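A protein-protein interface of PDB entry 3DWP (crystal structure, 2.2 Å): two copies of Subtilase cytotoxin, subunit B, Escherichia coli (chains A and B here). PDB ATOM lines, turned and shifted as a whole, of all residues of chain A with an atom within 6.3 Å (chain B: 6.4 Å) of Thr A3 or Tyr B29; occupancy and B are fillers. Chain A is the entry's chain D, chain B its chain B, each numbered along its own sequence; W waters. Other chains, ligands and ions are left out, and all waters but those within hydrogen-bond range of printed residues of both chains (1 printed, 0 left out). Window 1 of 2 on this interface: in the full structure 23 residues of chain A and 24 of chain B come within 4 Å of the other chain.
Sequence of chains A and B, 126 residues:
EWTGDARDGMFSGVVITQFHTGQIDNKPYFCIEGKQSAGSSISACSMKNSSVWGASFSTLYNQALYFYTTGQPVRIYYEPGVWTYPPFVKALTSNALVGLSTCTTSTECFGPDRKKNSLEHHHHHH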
ATOM      1  N   GLU A   1       9.924  14.096  12.762  1.00  0.00           N
ATOM      2  CA  GLU A   1      11.014  13.109  12.972  1.00  0.00           C
ATOM      3  C   GLU A   1      12.344  13.819  13.216  1.00  0.00           C
ATOM      4  O   GLU A   1      12.568  14.972  12.793  1.00  0.00           O
ATOM      5  CB  GLU A   1      11.125  12.179  11.754  1.00  0.00           C
ATOM      6  CG  GLU A   1      12.039  12.709  10.592  1.00  0.00           C
ATOM      7  CD  GLU A   1      11.530  13.973   9.920  1.00  0.00           C
ATOM      8  OE1 GLU A   1      12.240  14.491   9.041  1.00  0.00           O
ATOM      9  OE2 GLU A   1      10.432  14.470  10.269  1.00  0.00           O
ATOM     10  N   TRP A   2      13.230  13.106  13.892  1.00  0.00           N
ATOM     11  CA  TRP A   2      14.516  13.617  14.235  1.00  0.00           C
ATOM     12  C   TRP A   2      15.450  12.444  14.464  1.00  0.00           C
ATOM     13  O   TRP A   2      15.058  11.423  15.039  1.00  0.00           O
ATOM     14  CB  TRP A   2      14.426  14.523  15.481  1.00  0.00           C
ATOM     15  CG  TRP A   2      15.762  14.977  16.027  1.00  0.00           C
ATOM     16  CD1 TRP A   2      16.836  15.445  15.307  1.00  0.00           C
ATOM     17  CD2 TRP A   2      16.145  15.040  17.411  1.00  0.00           C
ATOM     18  NE1 TRP A   2      17.885  15.767  16.164  1.00  0.00           N
ATOM     19  CE2 TRP A   2      17.479  15.544  17.459  1.00  0.00           C
ATOM     20  CE3 TRP A   2      15.498  14.720  18.615  1.00  0.00           C
ATOM     21  CZ2 TRP A   2      18.182  15.709  18.668  1.00  0.00           C
ATOM     22  CZ3 TRP A   2      16.198  14.886  19.816  1.00  0.00           C
ATOM     23  CH2 TRP A   2      17.533  15.377  19.827  1.00  0.00           C
ATOM     24  N   THR A   3      16.694  12.605  14.000  1.00  0.00           N
ATOM     25  CA  THR A   3      17.793  11.706  14.315  1.00  0.00           C
ATOM     26  C   THR A   3      17.784  11.273  15.799  1.00  0.00           C
ATOM     27  O   THR A   3      17.985  10.088  16.142  1.00  0.00           O
ATOM     28  CB  THR A   3      19.123  12.408  13.941  1.00  0.00           C
ATOM     29  OG1 THR A   3      19.085  12.765  12.556  1.00  0.00           O
ATOM     30  CG2 THR A   3      20.286  11.535  14.189  1.00  0.00           C
ATOM     31  N   GLY A   4      17.513  12.222  16.681  1.00  0.00           N
ATOM     32  CA  GLY A   4      17.522  11.921  18.109  1.00  0.00           C
ATOM     33  C   GLY A   4      16.218  11.447  18.722  1.00  0.00           C
ATOM     34  O   GLY A   4      16.065  11.519  19.927  1.00  0.00           O
ATOM     35  N   ASP A   5      15.276  10.968  17.915  1.00  0.00           N
ATOM     36  CA  ASP A   5      14.051  10.363  18.456  1.00  0.00           C
ATOM     37  C   ASP A   5      14.388   9.133  19.259  1.00  0.00           C
ATOM     38  O   ASP A   5      15.362   8.436  18.946  1.00  0.00           O
ATOM     39  CB  ASP A   5      13.072   9.965  17.359  1.00  0.00           C
ATOM     40  CG  ASP A   5      12.409  11.144  16.716  1.00  0.00           C
ATOM     41  OD1 ASP A   5      12.289  12.204  17.354  1.00  0.00           O
ATOM     42  OD2 ASP A   5      11.997  11.010  15.556  1.00  0.00           O
ATOM     43  N   ALA A   6      13.568   8.867  20.278  1.00  0.00           N
ATOM     44  CA  ALA A   6      13.774   7.726  21.183  1.00  0.00           C
ATOM     45  C   ALA A   6      13.364   6.379  20.554  1.00  0.00           C
ATOM     46  O   ALA A   6      12.372   5.755  20.968  1.00  0.00           O
ATOM     47  CB  ALA A   6      13.079   7.965  22.541  1.00  0.00           C
ATOM     48  N   GLY A   9      17.893   3.159  15.880  1.00  0.00           N
ATOM     49  CA  GLY A   9      18.883   2.851  16.897  1.00  0.00           C
ATOM     50  C   GLY A   9      20.185   3.539  16.542  1.00  0.00           C
ATOM     51  O   GLY A   9      20.251   4.327  15.580  1.00  0.00           O
ATOM     52  N   MET A  10      21.229   3.219  17.296  1.00  0.00           N
ATOM     53  CA  MET A  10      22.557   3.738  17.016  1.00  0.00           C
ATOM     54  C   MET A  10      23.644   2.721  17.340  1.00  0.00           C
ATOM     55  O   MET A  10      23.469   1.894  18.223  1.00  0.00           O
ATOM     56  CB  MET A  10      22.783   5.033  17.785  1.00  0.00           C
ATOM     57  CG  MET A  10      22.555   4.851  19.254  1.00  0.00           C
ATOM     58  SD  MET A  10      22.968   6.267  20.219  1.00  0.00           S
ATOM     59  CE  MET A  10      22.518   7.550  19.132  1.00  0.00           C
ATOM     60  N   TRP A  53      13.805  10.222   5.297  1.00  0.00           N
ATOM     61  CA  TRP A  53      15.218  10.535   5.416  1.00  0.00           C
ATOM     62  C   TRP A  53      15.888  10.932   4.112  1.00  0.00           C
ATOM     63  O   TRP A  53      17.099  11.167   4.083  1.00  0.00           O
ATOM     64  CB  TRP A  53      15.954   9.379   6.081  1.00  0.00           C
ATOM     65  CG  TRP A  53      15.315   8.932   7.353  1.00  0.00           C
ATOM     66  CD1 TRP A  53      14.616   7.769   7.554  1.00  0.00           C
ATOM     67  CD2 TRP A  53      15.295   9.632   8.606  1.00  0.00           C
ATOM     68  NE1 TRP A  53      14.173   7.699   8.847  1.00  0.00           N
ATOM     69  CE2 TRP A  53      14.571   8.819   9.525  1.00  0.00           C
ATOM     70  CE3 TRP A  53      15.838  10.854   9.055  1.00  0.00           C
ATOM     71  CZ2 TRP A  53      14.362   9.191  10.866  1.00  0.00           C
ATOM     72  CZ3 TRP A  53      15.623  11.234  10.380  1.00  0.00           C
ATOM     73  CH2 TRP A  53      14.894  10.395  11.277  1.00  0.00           C
ATOM     74  N   SER A  56      18.308  14.223   3.667  1.00  0.00           N
ATOM     75  CA  SER A  56      19.640  14.135   4.238  1.00  0.00           C
ATOM     76  C   SER A  56      20.683  13.471   3.314  1.00  0.00           C
ATOM     77  O   SER A  56      21.866  13.448   3.658  1.00  0.00           O
ATOM     78  CB  SER A  56      19.566  13.255   5.481  1.00  0.00           C
ATOM     79  OG  SER A  56      19.009  13.934   6.563  1.00  0.00           O
ATOM     80  N   THR A  59      24.072  15.490   2.427  1.00  0.00           N
ATOM     81  CA  THR A  59      24.840  15.757   3.646  1.00  0.00           C
ATOM     82  C   THR A  59      25.477  14.497   4.196  1.00  0.00           C
ATOM     83  O   THR A  59      26.644  14.502   4.581  1.00  0.00           O
ATOM     84  CB  THR A  59      23.941  16.412   4.762  1.00  0.00           C
ATOM     85  OG1 THR A  59      23.376  17.625   4.264  1.00  0.00           O
ATOM     86  CG2 THR A  59      24.750  16.734   6.001  1.00  0.00           C
ATOM     87  N   TYR A  77      23.806   6.491  13.266  1.00  0.00           N
ATOM     88  CA  TYR A  77      22.372   6.515  13.579  1.00  0.00           C
ATOM     89  C   TYR A  77      21.590   5.887  12.424  1.00  0.00           C
ATOM     90  O   TYR A  77      21.787   6.251  11.264  1.00  0.00           O
ATOM     91  CB  TYR A  77      21.876   7.957  13.732  1.00  0.00           C
ATOM     92  CG  TYR A  77      22.505   8.767  14.834  1.00  0.00           C
ATOM     93  CD1 TYR A  77      21.864   8.889  16.067  1.00  0.00           C
ATOM     94  CD2 TYR A  77      23.724   9.465  14.636  1.00  0.00           C
ATOM     95  CE1 TYR A  77      22.405   9.660  17.089  1.00  0.00           C
ATOM     96  CE2 TYR A  77      24.275  10.242  15.664  1.00  0.00           C
ATOM     97  CZ  TYR A  77      23.597  10.330  16.890  1.00  0.00           C
ATOM     98  OH  TYR A  77      24.093  11.075  17.929  1.00  0.00           O
ATOM     99  N   VAL A  98      20.503   7.749   9.148  1.00  0.00           N
ATOM    100  CA  VAL A  98      19.703   8.911   9.618  1.00  0.00           C
ATOM    101  C   VAL A  98      20.517   9.996  10.329  1.00  0.00           C
ATOM    102  O   VAL A  98      19.999  11.069  10.627  1.00  0.00           O
ATOM    103  CB  VAL A  98      18.414   8.496  10.450  1.00  0.00           C
ATOM    104  CG1 VAL A  98      17.676   7.337   9.776  1.00  0.00           C
ATOM    105  CG2 VAL A  98      18.742   8.118  11.887  1.00  0.00           C
ATOM    106  N   GLY A  99      21.788   9.718  10.599  1.00  0.00           N
ATOM    107  CA  GLY A  99      22.704  10.742  11.052  1.00  0.00           C
ATOM    108  C   GLY A  99      24.084  10.154  11.281  1.00  0.00           C
ATOM    109  O   GLY A  99      24.255   8.947  11.178  1.00  0.00           O
ATOM    110  N   LEU A 100      25.052  11.016  11.607  1.00  0.00           N
ATOM    111  CA  LEU A 100      26.453  10.629  11.901  1.00  0.00           C
ATOM    112  C   LEU A 100      27.065  11.541  12.965  1.00  0.00           C
ATOM    113  O   LEU A 100      26.702  12.712  13.049  1.00  0.00           O
ATOM    114  CB  LEU A 100      27.316  10.699  10.615  1.00  0.00           C
ATOM    115  CG  LEU A 100      27.045   9.721   9.451  1.00  0.00           C
ATOM    116  CD1 LEU A 100      27.657  10.218   8.132  1.00  0.00           C
ATOM    117  CD2 LEU A 100      27.508   8.272   9.764  1.00  0.00           C
ATOM    118  N   PRO A 112      22.816  13.509  20.001  1.00  0.00           N
ATOM    119  CA  PRO A 112      21.739  12.838  20.731  1.00  0.00           C
ATOM    120  C   PRO A 112      21.930  11.316  20.840  1.00  0.00           C
ATOM    121  O   PRO A 112      22.653  10.696  20.054  1.00  0.00           O
ATOM    122  CB  PRO A 112      20.508  13.114  19.855  1.00  0.00           C
ATOM    123  CG  PRO A 112      21.067  13.232  18.474  1.00  0.00           C
ATOM    124  CD  PRO A 112      22.372  13.951  18.666  1.00  0.00           C
ATOM    125  N   ASP A 113      21.282  10.733  21.835  1.00  0.00           N
ATOM    126  CA  ASP A 113      21.081   9.301  21.852  1.00  0.00           C
ATOM    127  C   ASP A 113      19.923   9.013  20.903  1.00  0.00           C
ATOM    128  O   ASP A 113      19.058   9.845  20.705  1.00  0.00           O
ATOM    129  CB  ASP A 113      20.786   8.816  23.271  1.00  0.00           C
ATOM    130  CG  ASP A 113      21.999   8.898  24.175  1.00  0.00           C
ATOM    131  OD1 ASP A 113      23.141   8.897  23.669  1.00  0.00           O
ATOM    132  OD2 ASP A 113      21.814   8.966  25.407  1.00  0.00           O
ATOM    133  N   ARG A 114      19.950   7.860  20.265  1.00  0.00           N
ATOM    134  CA  ARG A 114      18.811   7.377  19.518  1.00  0.00           C
ATOM    135  C   ARG A 114      18.559   5.966  20.051  1.00  0.00           C
ATOM    136  O   ARG A 114      19.035   4.995  19.460  1.00  0.00           O
ATOM    137  CB  ARG A 114      19.120   7.376  18.016  1.00  0.00           C
ATOM    138  CG  ARG A 114      17.989   6.878  17.176  1.00  0.00           C
ATOM    139  CD  ARG A 114      18.244   6.977  15.714  1.00  0.00           C
ATOM    140  NE  ARG A 114      17.154   6.357  14.985  1.00  0.00           N
ATOM    141  CZ  ARG A 114      16.056   6.974  14.564  1.00  0.00           C
ATOM    142  NH1 ARG A 114      15.854   8.274  14.752  1.00  0.00           N
ATOM    143  NH2 ARG A 114      15.151   6.275  13.926  1.00  0.00           N
ATOM    144  N   HIS B  20      28.602  16.675  14.214  1.00  0.00           N
ATOM    145  CA  HIS B  20      27.421  15.836  14.161  1.00  0.00           C
ATOM    146  C   HIS B  20      26.523  16.296  13.021  1.00  0.00           C
ATOM    147  O   HIS B  20      26.437  17.480  12.723  1.00  0.00           O
ATOM    148  CB  HIS B  20      26.633  15.871  15.469  1.00  0.00           C
ATOM    149  CG  HIS B  20      25.309  15.184  15.376  1.00  0.00           C
ATOM    150  ND1 HIS B  20      24.116  15.866  15.416  1.00  0.00           N
ATOM    151  CD2 HIS B  20      24.992  13.884  15.200  1.00  0.00           C
ATOM    152  CE1 HIS B  20      23.117  15.013  15.284  1.00  0.00           C
ATOM    153  NE2 HIS B  20      23.623  13.805  15.130  1.00  0.00           N
ATOM    154  N   THR B  21      25.860  15.325  12.407  1.00  0.00           N
ATOM    155  CA  THR B  21      25.068  15.507  11.214  1.00  0.00           C
ATOM    156  C   THR B  21      23.795  14.669  11.443  1.00  0.00           C
ATOM    157  O   THR B  21      23.870  13.531  11.885  1.00  0.00           O
ATOM    158  CB  THR B  21      25.938  15.080   9.989  1.00  0.00           C
ATOM    159  OG1 THR B  21      26.374  16.244   9.279  1.00  0.00           O
ATOM    160  CG2 THR B  21      25.237  14.150   9.044  1.00  0.00           C
ATOM    161  N   GLY B  22      22.632  15.251  11.199  1.00  0.00           N
ATOM    162  CA  GLY B  22      21.380  14.547  11.365  1.00  0.00           C
ATOM    163  C   GLY B  22      20.291  15.204  10.540  1.00  0.00           C
ATOM    164  O   GLY B  22      20.579  15.992   9.650  1.00  0.00           O
ATOM    165  N   GLN B  23      19.041  14.852  10.818  1.00  0.00           N
ATOM    166  CA  GLN B  23      17.891  15.453  10.142  1.00  0.00           C
ATOM    167  C   GLN B  23      16.779  15.701  11.159  1.00  0.00           C
ATOM    168  O   GLN B  23      16.622  14.929  12.106  1.00  0.00           O
ATOM    169  CB  GLN B  23      17.364  14.532   9.026  1.00  0.00           C
ATOM    170  CG  GLN B  23      16.054  15.006   8.360  1.00  0.00           C
ATOM    171  CD  GLN B  23      15.533  14.053   7.269  1.00  0.00           C
ATOM    172  OE1 GLN B  23      16.295  13.601   6.417  1.00  0.00           O
ATOM    173  NE2 GLN B  23      14.226  13.755   7.298  1.00  0.00           N
ATOM    174  N   ILE B  24      16.006  16.773  10.932  1.00  0.00           N
ATOM    175  CA  ILE B  24      14.807  17.084  11.705  1.00  0.00           C
ATOM    176  C   ILE B  24      13.801  17.766  10.767  1.00  0.00           C
ATOM    177  O   ILE B  24      14.169  18.678   9.994  1.00  0.00           O
ATOM    178  CB  ILE B  24      15.096  17.943  13.000  1.00  0.00           C
ATOM    179  CG1 ILE B  24      13.813  18.119  13.854  1.00  0.00           C
ATOM    180  CG2 ILE B  24      15.670  19.310  12.640  1.00  0.00           C
ATOM    181  CD1 ILE B  24      14.046  18.478  15.360  1.00  0.00           C
ATOM    182  N   LYS B  27      14.644  18.274   7.146  1.00  0.00           N
ATOM    183  CA  LYS B  27      15.805  19.155   6.964  1.00  0.00           C
ATOM    184  C   LYS B  27      17.098  18.607   7.549  1.00  0.00           C
ATOM    185  O   LYS B  27      17.177  18.367   8.740  1.00  0.00           O
ATOM    186  CB  LYS B  27      15.576  20.528   7.597  1.00  0.00           C
ATOM    187  CG  LYS B  27      14.529  21.365   6.942  1.00  0.00           C
ATOM    188  CD  LYS B  27      14.144  22.492   7.872  1.00  0.00           C
ATOM    189  CE  LYS B  27      12.929  23.212   7.361  1.00  0.00           C
ATOM    190  NZ  LYS B  27      13.280  24.037   6.205  1.00  0.00           N
ATOM    191  N   PRO B  28      18.143  18.493   6.714  1.00  0.00           N
ATOM    192  CA  PRO B  28      19.458  18.133   7.233  1.00  0.00           C
ATOM    193  C   PRO B  28      20.028  19.304   8.051  1.00  0.00           C
ATOM    194  O   PRO B  28      19.796  20.472   7.732  1.00  0.00           O
ATOM    195  CB  PRO B  28      20.290  17.889   5.968  1.00  0.00           C
ATOM    196  CG  PRO B  28      19.635  18.760   4.898  1.00  0.00           C
ATOM    197  CD  PRO B  28      18.152  18.760   5.254  1.00  0.00           C
ATOM    198  N   TYR B  29      20.754  18.986   9.114  1.00  0.00           N
ATOM    199  CA  TYR B  29      21.399  20.017   9.905  1.00  0.00           C
ATOM    200  C   TYR B  29      22.755  19.416  10.274  1.00  0.00           C
ATOM    201  O   TYR B  29      22.927  18.193  10.232  1.00  0.00           O
ATOM    202  CB  TYR B  29      20.553  20.356  11.170  1.00  0.00           C
ATOM    203  CG  TYR B  29      20.521  19.210  12.156  1.00  0.00           C
ATOM    204  CD1 TYR B  29      21.548  19.052  13.087  1.00  0.00           C
ATOM    205  CD2 TYR B  29      19.493  18.250  12.127  1.00  0.00           C
ATOM    206  CE1 TYR B  29      21.551  17.994  13.967  1.00  0.00           C
ATOM    207  CE2 TYR B  29      19.497  17.176  13.026  1.00  0.00           C
ATOM    208  CZ  TYR B  29      20.527  17.053  13.930  1.00  0.00           C
ATOM    209  OH  TYR B  29      20.579  15.993  14.825  1.00  0.00           O
ATOM    210  N   PHE B  30      23.726  20.264  10.596  1.00  0.00           N
ATOM    211  CA  PHE B  30      24.917  19.772  11.238  1.00  0.00           C
ATOM    212  C   PHE B  30      25.062  20.598  12.484  1.00  0.00           C
ATOM    213  O   PHE B  30      24.444  21.661  12.651  1.00  0.00           O
ATOM    214  CB  PHE B  30      26.185  19.848  10.372  1.00  0.00           C
ATOM    215  CG  PHE B  30      26.712  21.251  10.182  1.00  0.00           C
ATOM    216  CD1 PHE B  30      27.738  21.747  11.006  1.00  0.00           C
ATOM    217  CD2 PHE B  30      26.188  22.074   9.174  1.00  0.00           C
ATOM    218  CE1 PHE B  30      28.201  23.020  10.836  1.00  0.00           C
ATOM    219  CE2 PHE B  30      26.657  23.358   9.006  1.00  0.00           C
ATOM    220  CZ  PHE B  30      27.657  23.836   9.827  1.00  0.00           C
ATOM    221  N   CYS B  31      25.885  20.083  13.367  1.00  0.00           N
ATOM    222  CA  CYS B  31      26.071  20.696  14.627  1.00  0.00           C
ATOM    223  C   CYS B  31      27.587  20.500  14.939  1.00  0.00           C
ATOM    224  O   CYS B  31      28.180  19.503  14.554  1.00  0.00           O
ATOM    225  CB  CYS B  31      25.025  20.093  15.617  1.00  0.00           C
ATOM    226  SG  CYS B  31      24.630  21.242  16.875  1.00  0.00           S
ATOM    227  N   CYS B  45      24.516  24.884  15.846  1.00  0.00           N
ATOM    228  CA  CYS B  45      24.044  24.103  14.697  1.00  0.00           C
ATOM    229  C   CYS B  45      23.603  24.984  13.573  1.00  0.00           C
ATOM    230  O   CYS B  45      23.035  26.066  13.791  1.00  0.00           O
ATOM    231  CB  CYS B  45      22.867  23.153  15.004  1.00  0.00           C
ATOM    232  SG  CYS B  45      22.859  22.204  16.544  1.00  0.00           S
ATOM    233  N   SER B  46      23.859  24.492  12.363  1.00  0.00           N
ATOM    234  CA  SER B  46      23.253  25.053  11.184  1.00  0.00           C
ATOM    235  C   SER B  46      22.273  24.043  10.581  1.00  0.00           C
ATOM    236  O   SER B  46      22.526  22.851  10.603  1.00  0.00           O
ATOM    237  CB  SER B  46      24.329  25.472  10.189  1.00  0.00           C
ATOM    238  OG  SER B  46      23.751  26.152   9.109  1.00  0.00           O
ATOM    239  N   MET B  47      21.165  24.535  10.039  1.00  0.00           N
ATOM    240  CA  MET B  47      20.124  23.677   9.493  1.00  0.00           C
ATOM    241  C   MET B  47      19.691  24.175   8.122  1.00  0.00           C
ATOM    242  O   MET B  47      19.350  25.360   7.974  1.00  0.00           O
ATOM    243  CB  MET B  47      18.928  23.667  10.449  1.00  0.00           C
ATOM    244  CG  MET B  47      17.799  22.695  10.078  1.00  0.00           C
ATOM    245  SD  MET B  47      16.438  22.849  11.252  1.00  0.00           S
ATOM    246  CE  MET B  47      17.236  22.438  12.806  1.00  0.00           C
ATOM    247  N   LYS B  48      19.681  23.276   7.132  1.00  0.00           N
ATOM    248  CA  LYS B  48      19.261  23.632   5.768  1.00  0.00           C
ATOM    249  C   LYS B  48      17.866  24.221   5.754  1.00  0.00           C
ATOM    250  O   LYS B  48      16.952  23.671   6.389  1.00  0.00           O
ATOM    251  CB  LYS B  48      19.287  22.426   4.844  1.00  0.00           C
ATOM    252  CG  LYS B  48      19.058  22.767   3.364  1.00  0.00           C
ATOM    253  CD  LYS B  48      19.276  21.524   2.517  1.00  0.00           C
ATOM    254  CE  LYS B  48      18.914  21.701   1.066  1.00  0.00           C
ATOM    255  NZ  LYS B  48      19.043  20.359   0.400  1.00  0.00           N
ATOM    256  N   PHE B  57      23.489  27.562   5.423  1.00  0.00           N
ATOM    257  CA  PHE B  57      23.781  26.127   5.665  1.00  0.00           C
ATOM    258  C   PHE B  57      24.970  25.543   4.879  1.00  0.00           C
ATOM    259  O   PHE B  57      25.915  25.002   5.473  1.00  0.00           O
ATOM    260  CB  PHE B  57      22.540  25.248   5.446  1.00  0.00           C
ATOM    261  CG  PHE B  57      22.808  23.780   5.648  1.00  0.00           C
ATOM    262  CD1 PHE B  57      22.948  23.258   6.928  1.00  0.00           C
ATOM    263  CD2 PHE B  57      22.947  22.916   4.547  1.00  0.00           C
ATOM    264  CE1 PHE B  57      23.204  21.859   7.125  1.00  0.00           C
ATOM    265  CE2 PHE B  57      23.234  21.541   4.731  1.00  0.00           C
ATOM    266  CZ  PHE B  57      23.352  21.015   6.030  1.00  0.00           C
ATOM    267  N   PHE B  88      15.804  18.418  21.123  1.00  0.00           N
ATOM    268  CA  PHE B  88      16.938  18.861  20.289  1.00  0.00           C
ATOM    269  C   PHE B  88      17.829  19.817  21.071  1.00  0.00           C
ATOM    270  O   PHE B  88      19.052  19.680  21.069  1.00  0.00           O
ATOM    271  CB  PHE B  88      16.415  19.499  18.982  1.00  0.00           C
ATOM    272  CG  PHE B  88      17.491  19.989  18.034  1.00  0.00           C
ATOM    273  CD1 PHE B  88      17.708  19.326  16.819  1.00  0.00           C
ATOM    274  CD2 PHE B  88      18.240  21.152  18.312  1.00  0.00           C
ATOM    275  CE1 PHE B  88      18.676  19.790  15.903  1.00  0.00           C
ATOM    276  CE2 PHE B  88      19.220  21.617  17.406  1.00  0.00           C
ATOM    277  CZ  PHE B  88      19.446  20.935  16.199  1.00  0.00           C
ATOM    278  N   LEU B  92      21.636  18.791  22.196  1.00  0.00           N
ATOM    279  CA  LEU B  92      22.517  19.583  21.361  1.00  0.00           C
ATOM    280  C   LEU B  92      22.653  20.988  21.917  1.00  0.00           C
ATOM    281  O   LEU B  92      23.425  21.212  22.833  1.00  0.00           O
ATOM    282  CB  LEU B  92      22.028  19.593  19.895  1.00  0.00           C
ATOM    283  CG  LEU B  92      22.184  18.228  19.162  1.00  0.00           C
ATOM    284  CD1 LEU B  92      21.468  18.221  17.807  1.00  0.00           C
ATOM    285  CD2 LEU B  92      23.655  17.862  18.991  1.00  0.00           C
HETATM  286  O   HOH W   1      20.303  12.566   8.503  1.00  0.00           O
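Of the 17 printed residues of chain B, 9 touch a printed residue of chain A. Hydrophobic or aromatic side chains of chain B that line the printed part of chain A: His B20, Ile B24, Pro B28, Tyr B29, Phe B57 and Phe B88. Along chain B the printed residues that touch a printed residue of chain A span positions 20 to 88. Of the 18 printed residues of chain A, 11 touch a printed residue of chain B.
No position is printed for both chains. Of the 21 pairs that touch across the chains among the printed residues, none has its exchanged pair printed and touching as well.
Water W1 lies within hydrogen-bond range of the backbone carbonyl oxygen of Val A98, the side-chain hydroxyl of Ser A56 and the backbone NH of Gln B23.
Thr A3 touches just these residues of chain B: Gly B22 (3.1 Å), Gln B23 (2.7 Å) and Tyr B29 (3.97 Å). Printed residues of chain B within 4 Å of Leu A100: His B20 and Thr B21. Printed residues of chain B within 4 Å of Pro A112: His B20 (3.6 Å). Of the printed residues of chain A, His B20 touches Tyr A77 (3.7 Å), Leu A100 (3.0 Å) and Pro A112 (3.6 Å). Of the printed residues of chain A, Gly B22 touches Thr A3 and Val A98. Tyr B29 touches two residues of chain A. Printed residues of chain A within 4 Å of Phe B88: Trp A2 (3.6 Å). The nearest residue of chain B that does not touch Thr A3 is His B20 (4.1 Å). The nearest residue of chain A that does not touch Tyr B29 is Pro A112 (4.6 Å). The nearest printed residue of chain A that does not touch Thr B21 is Thr A3 (4.7 Å).
Among the printed residues, pairs that only touch across the chains: Glu A1 with Ile B24, Trp A2 with Gln B23, Trp A2 with Ile B24, Trp A2 with Phe B88, Thr A3 with Gly B22, Thr A3 with Tyr B29, Thr A59 with Thr B21, Thr A59 with Pro B28, Thr A59 with Phe B57, Tyr A77 with His B20, Val A98 with Gly B22, Val A98 with Gln B23, Gly A99 with Thr B21, Leu A100 with His B20 and Pro A112 with His B20.
N of Gln B23 is in hydrogen-bond range of OG1 of Thr A3 (2.7 Å). The backbone carbonyl oxygen (O) of Trp A53 lies close to the side-chain amide oxygen (OE1) of Gln B23 (3.5 Å). NE1 of Trp A2 sits at hydrogen-bond distance from OH of Tyr B29 (3.0 Å). OG of Ser A56 is in hydrogen-bond range of OE1 of Gln B23. N of Leu A100 is in hydrogen-bond range of O of Thr B21 (2.8 Å). The side-chain amide nitrogen (NE2) of Gln B23 lies within hydrogen-bond range of the side-chain carboxylate (OE1) of Glu A1.
The backbone NH (N) of Tyr A77 is in hydrogen-bond range of the backbone carbonyl oxygen (O) of Gly A99 (3.3 Å). The backbone carbonyl oxygen of Thr A3 lies within hydrogen-bond range of the guanidinium group of Arg A114 (3.1 Å). The backbone NH of Trp A2 is in hydrogen-bond range of the side-chain carboxylate of Asp A5 (2.9 Å). The backbone carbonyl oxygen (O) of Pro B28 sits at hydrogen-bond distance from the backbone NH (N) of Lys B48, at 2.9 Å. O of Pro A112 sits at hydrogen-bond distance from OH of Tyr A77, 2.6 Å away. The backbone NH (N) of Val A98 sits at hydrogen-bond distance from the backbone carbonyl oxygen (O) of Tyr A77 (2.9 Å).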
